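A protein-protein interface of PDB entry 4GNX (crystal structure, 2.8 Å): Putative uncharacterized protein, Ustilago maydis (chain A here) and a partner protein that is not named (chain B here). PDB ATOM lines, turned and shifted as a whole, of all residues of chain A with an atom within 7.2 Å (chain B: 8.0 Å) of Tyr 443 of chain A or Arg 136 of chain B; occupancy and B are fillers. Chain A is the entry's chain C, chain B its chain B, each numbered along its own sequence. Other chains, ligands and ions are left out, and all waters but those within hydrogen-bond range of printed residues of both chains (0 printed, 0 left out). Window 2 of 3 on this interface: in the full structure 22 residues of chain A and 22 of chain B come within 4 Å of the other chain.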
ATOM      1  N   ALA A  84      14.350  17.751  34.391  1.00  0.00           N
ATOM      2  CA  ALA A  84      15.230  16.991  35.265  1.00  0.00           C
ATOM      3  C   ALA A  84      16.115  16.069  34.444  1.00  0.00           C
ATOM      4  O   ALA A  84      15.650  15.485  33.465  1.00  0.00           O
ATOM      5  CB  ALA A  84      14.417  16.198  36.259  1.00  0.00           C
ATOM      6  N   LYS A  86      17.382  12.804  35.120  1.00  0.00           N
ATOM      7  CA  LYS A  86      17.204  11.741  36.118  1.00  0.00           C
ATOM      8  C   LYS A  86      18.364  10.738  36.213  1.00  0.00           C
ATOM      9  O   LYS A  86      18.486  10.022  37.213  1.00  0.00           O
ATOM     10  CB  LYS A  86      15.873  11.026  35.889  1.00  0.00           C
ATOM     11  CG  LYS A  86      14.685  11.893  36.246  1.00  0.00           C
ATOM     12  CD  LYS A  86      13.462  11.418  35.505  1.00  0.00           C
ATOM     13  CE  LYS A  86      12.250  12.225  35.900  1.00  0.00           C
ATOM     14  NZ  LYS A  86      11.035  11.557  35.365  1.00  0.00           N
ATOM     15  N   GLN A  87      19.222  10.705  35.196  1.00  0.00           N
ATOM     16  CA  GLN A  87      20.443   9.891  35.257  1.00  0.00           C
ATOM     17  C   GLN A  87      21.355  10.337  36.398  1.00  0.00           C
ATOM     18  O   GLN A  87      22.212   9.579  36.856  1.00  0.00           O
ATOM     19  CB  GLN A  87      21.206   9.954  33.940  1.00  0.00           C
ATOM     20  CG  GLN A  87      20.292   9.848  32.746  1.00  0.00           C
ATOM     21  CD  GLN A  87      20.853   9.002  31.621  1.00  0.00           C
ATOM     22  OE1 GLN A  87      21.252   7.843  31.816  1.00  0.00           O
ATOM     23  NE2 GLN A  87      20.867   9.576  30.422  1.00  0.00           N
ATOM     24  N   VAL A 437      13.198  -1.355  33.450  1.00  0.00           N
ATOM     25  CA  VAL A 437      12.268  -0.237  33.594  1.00  0.00           C
ATOM     26  C   VAL A 437      12.943   0.905  34.324  1.00  0.00           C
ATOM     27  O   VAL A 437      13.013   2.017  33.799  1.00  0.00           O
ATOM     28  CB  VAL A 437      10.981  -0.610  34.308  1.00  0.00           C
ATOM     29  CG1 VAL A 437      10.044   0.575  34.337  1.00  0.00           C
ATOM     30  CG2 VAL A 437      10.301  -1.735  33.563  1.00  0.00           C
ATOM     31  N   ASP A 438      13.481   0.614  35.504  1.00  0.00           N
ATOM     32  CA  ASP A 438      14.180   1.618  36.285  1.00  0.00           C
ATOM     33  C   ASP A 438      15.226   2.267  35.421  1.00  0.00           C
ATOM     34  O   ASP A 438      15.325   3.476  35.375  1.00  0.00           O
ATOM     35  CB  ASP A 438      14.879   0.993  37.492  1.00  0.00           C
ATOM     36  CG  ASP A 438      13.918   0.568  38.592  1.00  0.00           C
ATOM     37  OD1 ASP A 438      12.751   1.032  38.622  1.00  0.00           O
ATOM     38  OD2 ASP A 438      14.347  -0.247  39.447  1.00  0.00           O
ATOM     39  N   ALA A 439      16.002   1.456  34.719  1.00  0.00           N
ATOM     40  CA  ALA A 439      17.132   1.971  33.970  1.00  0.00           C
ATOM     41  C   ALA A 439      16.642   2.962  32.917  1.00  0.00           C
ATOM     42  O   ALA A 439      17.156   4.059  32.807  1.00  0.00           O
ATOM     43  CB  ALA A 439      17.919   0.828  33.346  1.00  0.00           C
ATOM     44  N   ILE A 440      15.611   2.566  32.180  1.00  0.00           N
ATOM     45  CA  ILE A 440      14.985   3.392  31.138  1.00  0.00           C
ATOM     46  C   ILE A 440      14.347   4.711  31.635  1.00  0.00           C
ATOM     47  O   ILE A 440      14.600   5.792  31.068  1.00  0.00           O
ATOM     48  CB  ILE A 440      13.975   2.561  30.314  1.00  0.00           C
ATOM     49  CG1 ILE A 440      14.694   1.408  29.601  1.00  0.00           C
ATOM     50  CG2 ILE A 440      13.262   3.437  29.308  1.00  0.00           C
ATOM     51  CD1 ILE A 440      13.796   0.331  29.050  1.00  0.00           C
ATOM     52  N   ARG A 441      13.538   4.626  32.690  1.00  0.00           N
ATOM     53  CA  ARG A 441      12.898   5.822  33.250  1.00  0.00           C
ATOM     54  C   ARG A 441      13.903   6.935  33.555  1.00  0.00           C
ATOM     55  O   ARG A 441      13.540   8.114  33.568  1.00  0.00           O
ATOM     56  CB  ARG A 441      12.111   5.491  34.514  1.00  0.00           C
ATOM     57  CG  ARG A 441      10.932   4.567  34.296  1.00  0.00           C
ATOM     58  CD  ARG A 441       9.703   5.329  33.854  1.00  0.00           C
ATOM     59  NE  ARG A 441       8.522   4.468  33.742  1.00  0.00           N
ATOM     60  CZ  ARG A 441       7.419   4.788  33.065  1.00  0.00           C
ATOM     61  NH1 ARG A 441       7.348   5.967  32.441  1.00  0.00           N
ATOM     62  NH2 ARG A 441       6.397   3.929  33.007  1.00  0.00           N
ATOM     63  N   ALA A 442      15.161   6.557  33.797  1.00  0.00           N
ATOM     64  CA  ALA A 442      16.246   7.521  34.033  1.00  0.00           C
ATOM     65  C   ALA A 442      16.640   8.335  32.783  1.00  0.00           C
ATOM     66  O   ALA A 442      17.218   9.409  32.918  1.00  0.00           O
ATOM     67  CB  ALA A 442      17.455   6.835  34.632  1.00  0.00           C
ATOM     68  N   TYR A 443      16.317   7.829  31.594  1.00  0.00           N
ATOM     69  CA  TYR A 443      16.464   8.571  30.352  1.00  0.00           C
ATOM     70  C   TYR A 443      15.177   9.310  29.964  1.00  0.00           C
ATOM     71  O   TYR A 443      15.146  10.013  28.962  1.00  0.00           O
ATOM     72  CB  TYR A 443      16.812   7.620  29.203  1.00  0.00           C
ATOM     73  CG  TYR A 443      18.156   6.948  29.308  1.00  0.00           C
ATOM     74  CD1 TYR A 443      18.295   5.713  29.963  1.00  0.00           C
ATOM     75  CD2 TYR A 443      19.295   7.529  28.735  1.00  0.00           C
ATOM     76  CE1 TYR A 443      19.533   5.083  30.053  1.00  0.00           C
ATOM     77  CE2 TYR A 443      20.532   6.910  28.824  1.00  0.00           C
ATOM     78  CZ  TYR A 443      20.647   5.691  29.485  1.00  0.00           C
ATOM     79  OH  TYR A 443      21.874   5.067  29.585  1.00  0.00           O
ATOM     80  N   MET A 444      14.105   9.112  30.724  1.00  0.00           N
ATOM     81  CA  MET A 444      12.844   9.830  30.483  1.00  0.00           C
ATOM     82  C   MET A 444      12.381  10.574  31.735  1.00  0.00           C
ATOM     83  O   MET A 444      12.451  11.791  31.817  1.00  0.00           O
ATOM     84  CB  MET A 444      11.743   8.860  30.111  1.00  0.00           C
ATOM     85  CG  MET A 444      12.098   7.798  29.095  1.00  0.00           C
ATOM     86  SD  MET A 444      10.939   6.416  29.275  1.00  0.00           S
ATOM     87  CE  MET A 444       9.364   7.256  29.498  1.00  0.00           C
ATOM     88  N   VAL B 128      14.992  -1.004  23.861  1.00  0.00           N
ATOM     89  CA  VAL B 128      14.971   0.403  24.272  1.00  0.00           C
ATOM     90  C   VAL B 128      16.309   0.707  24.946  1.00  0.00           C
ATOM     91  O   VAL B 128      17.070   1.605  24.515  1.00  0.00           O
ATOM     92  CB  VAL B 128      13.758   0.731  25.180  1.00  0.00           C
ATOM     93  CG1 VAL B 128      13.813   2.155  25.695  1.00  0.00           C
ATOM     94  CG2 VAL B 128      12.461   0.531  24.407  1.00  0.00           C
ATOM     95  N   HIS B 129      16.621  -0.065  25.977  1.00  0.00           N
ATOM     96  CA  HIS B 129      17.840   0.172  26.736  1.00  0.00           C
ATOM     97  C   HIS B 129      19.061   0.200  25.863  1.00  0.00           C
ATOM     98  O   HIS B 129      19.888   1.104  25.973  1.00  0.00           O
ATOM     99  CB  HIS B 129      17.990  -0.849  27.866  1.00  0.00           C
ATOM    100  CG  HIS B 129      19.159  -0.574  28.758  1.00  0.00           C
ATOM    101  ND1 HIS B 129      19.176   0.451  29.623  1.00  0.00           N
ATOM    102  CD2 HIS B 129      20.389  -1.188  28.851  1.00  0.00           C
ATOM    103  CE1 HIS B 129      20.356   0.489  30.259  1.00  0.00           C
ATOM    104  NE2 HIS B 129      21.104  -0.506  29.781  1.00  0.00           N
ATOM    105  N   ALA B 130      19.181  -0.772  24.968  1.00  0.00           N
ATOM    106  CA  ALA B 130      20.326  -0.790  24.062  1.00  0.00           C
ATOM    107  C   ALA B 130      20.379   0.495  23.242  1.00  0.00           C
ATOM    108  O   ALA B 130      21.372   1.204  23.309  1.00  0.00           O
ATOM    109  CB  ALA B 130      20.313  -2.023  23.182  1.00  0.00           C
ATOM    110  N   HIS B 131      19.283   0.823  22.541  1.00  0.00           N
ATOM    111  CA  HIS B 131      19.155   2.045  21.731  1.00  0.00           C
ATOM    112  C   HIS B 131      19.523   3.274  22.485  1.00  0.00           C
ATOM    113  O   HIS B 131      20.189   4.153  21.953  1.00  0.00           O
ATOM    114  CB  HIS B 131      17.737   2.179  21.201  1.00  0.00           C
ATOM    115  CG  HIS B 131      17.451   3.501  20.548  1.00  0.00           C
ATOM    116  ND1 HIS B 131      16.759   4.482  21.177  1.00  0.00           N
ATOM    117  CD2 HIS B 131      17.798   4.001  19.290  1.00  0.00           C
ATOM    118  CE1 HIS B 131      16.669   5.558  20.360  1.00  0.00           C
ATOM    119  NE2 HIS B 131      17.306   5.261  19.204  1.00  0.00           N
ATOM    120  N   LEU B 132      19.095   3.341  23.739  1.00  0.00           N
ATOM    121  CA  LEU B 132      19.439   4.467  24.575  1.00  0.00           C
ATOM    122  C   LEU B 132      20.916   4.564  24.862  1.00  0.00           C
ATOM    123  O   LEU B 132      21.446   5.648  24.988  1.00  0.00           O
ATOM    124  CB  LEU B 132      18.681   4.411  25.877  1.00  0.00           C
ATOM    125  CG  LEU B 132      17.269   4.968  25.789  1.00  0.00           C
ATOM    126  CD1 LEU B 132      16.503   4.623  27.059  1.00  0.00           C
ATOM    127  CD2 LEU B 132      17.312   6.475  25.541  1.00  0.00           C
ATOM    128  N   GLN B 133      21.592   3.433  24.958  1.00  0.00           N
ATOM    129  CA  GLN B 133      22.991   3.447  25.340  1.00  0.00           C
ATOM    130  C   GLN B 133      23.940   3.760  24.191  1.00  0.00           C
ATOM    131  O   GLN B 133      25.028   4.303  24.417  1.00  0.00           O
ATOM    132  CB  GLN B 133      23.354   2.153  26.033  1.00  0.00           C
ATOM    133  CG  GLN B 133      22.684   2.045  27.386  1.00  0.00           C
ATOM    134  CD  GLN B 133      23.660   1.608  28.447  1.00  0.00           C
ATOM    135  OE1 GLN B 133      24.283   0.546  28.337  1.00  0.00           O
ATOM    136  NE2 GLN B 133      23.818   2.430  29.479  1.00  0.00           N
ATOM    137  N   VAL B 134      23.530   3.437  22.968  1.00  0.00           N
ATOM    138  CA  VAL B 134      24.303   3.783  21.774  1.00  0.00           C
ATOM    139  C   VAL B 134      24.060   5.230  21.390  1.00  0.00           C
ATOM    140  O   VAL B 134      24.835   5.813  20.648  1.00  0.00           O
ATOM    141  CB  VAL B 134      23.910   2.958  20.533  1.00  0.00           C
ATOM    142  CG1 VAL B 134      25.157   2.574  19.763  1.00  0.00           C
ATOM    143  CG2 VAL B 134      23.138   1.712  20.906  1.00  0.00           C
ATOM    144  N   THR B 135      22.984   5.797  21.913  1.00  0.00           N
ATOM    145  CA  THR B 135      22.429   7.069  21.457  1.00  0.00           C
ATOM    146  C   THR B 135      22.675   8.196  22.456  1.00  0.00           C
ATOM    147  O   THR B 135      22.927   9.338  22.066  1.00  0.00           O
ATOM    148  CB  THR B 135      20.908   6.880  21.162  1.00  0.00           C
ATOM    149  OG1 THR B 135      20.711   6.714  19.751  1.00  0.00           O
ATOM    150  CG2 THR B 135      20.018   8.026  21.700  1.00  0.00           C
ATOM    151  N   ARG B 136      22.605   7.846  23.740  1.00  0.00           N
ATOM    152  CA  ARG B 136      22.585   8.787  24.848  1.00  0.00           C
ATOM    153  C   ARG B 136      21.273   9.568  24.849  1.00  0.00           C
ATOM    154  O   ARG B 136      20.214   9.020  25.148  1.00  0.00           O
ATOM    155  CB  ARG B 136      23.805   9.728  24.803  1.00  0.00           C
ATOM    156  CG  ARG B 136      24.592   9.811  26.111  1.00  0.00           C
ATOM    157  CD  ARG B 136      24.995   8.431  26.645  1.00  0.00           C
ATOM    158  NE  ARG B 136      25.247   7.465  25.567  1.00  0.00           N
ATOM    159  CZ  ARG B 136      26.377   7.379  24.870  1.00  0.00           C
ATOM    160  NH1 ARG B 136      27.393   8.203  25.131  1.00  0.00           N
ATOM    161  NH2 ARG B 136      26.491   6.473  23.908  1.00  0.00           N
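The side-chain hydroxyl (OH) of Tyr 443 of chain A sits at hydrogen-bond distance from the side-chain amide nitrogen (NE2) of Gln 133 of chain B (3.3 Å).
The guanidinium group (NH2) of Arg 136 of chain B is in hydrogen-bond range of the backbone carbonyl oxygen (O) of Gln 133 of chain B (2.7 Å).
Among the printed residues, pairs that only touch across the chains: Ala 439 of chain A with His 129 of chain B, Ile 440 of chain A with Val 128 of chain B, Tyr 443 of chain A with Leu 132 of chain B and Tyr 443 of chain A with Arg 136 of chain B.
Of the printed residues of chain B, Ile 440 of chain A touches Val 128. Printed residues of chain B within 4 Å of Tyr 443 of chain A: Leu 132, Gln 133 and Arg 136. Of the printed residues of chain A, His 129 of chain B touches Ala 439 (3.9 Å). Of the printed residues of chain A, Leu 132 of chain B touches Tyr 443 (3.6 Å). Of the printed residues of chain A, Gln 133 of chain B touches Tyr 443 (3.3 Å). Of the printed residues of chain A, Arg 136 of chain B touches Tyr 443 (3.99 Å). The nearest printed residue of chain B that does not touch Tyr 443 of chain A is His 129 of chain B (4.7 Å).
Printed residues of chain B that touch a printed residue of chain A: Val 128, His 129, Leu 132, Gln 133 and Arg 136. Hydrophobic or aromatic side chains of chain A that line the printed part of chain B: Ala 439, Ile 440 and Tyr 443. Among the printed residues, 5 pairs touch across the chains.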
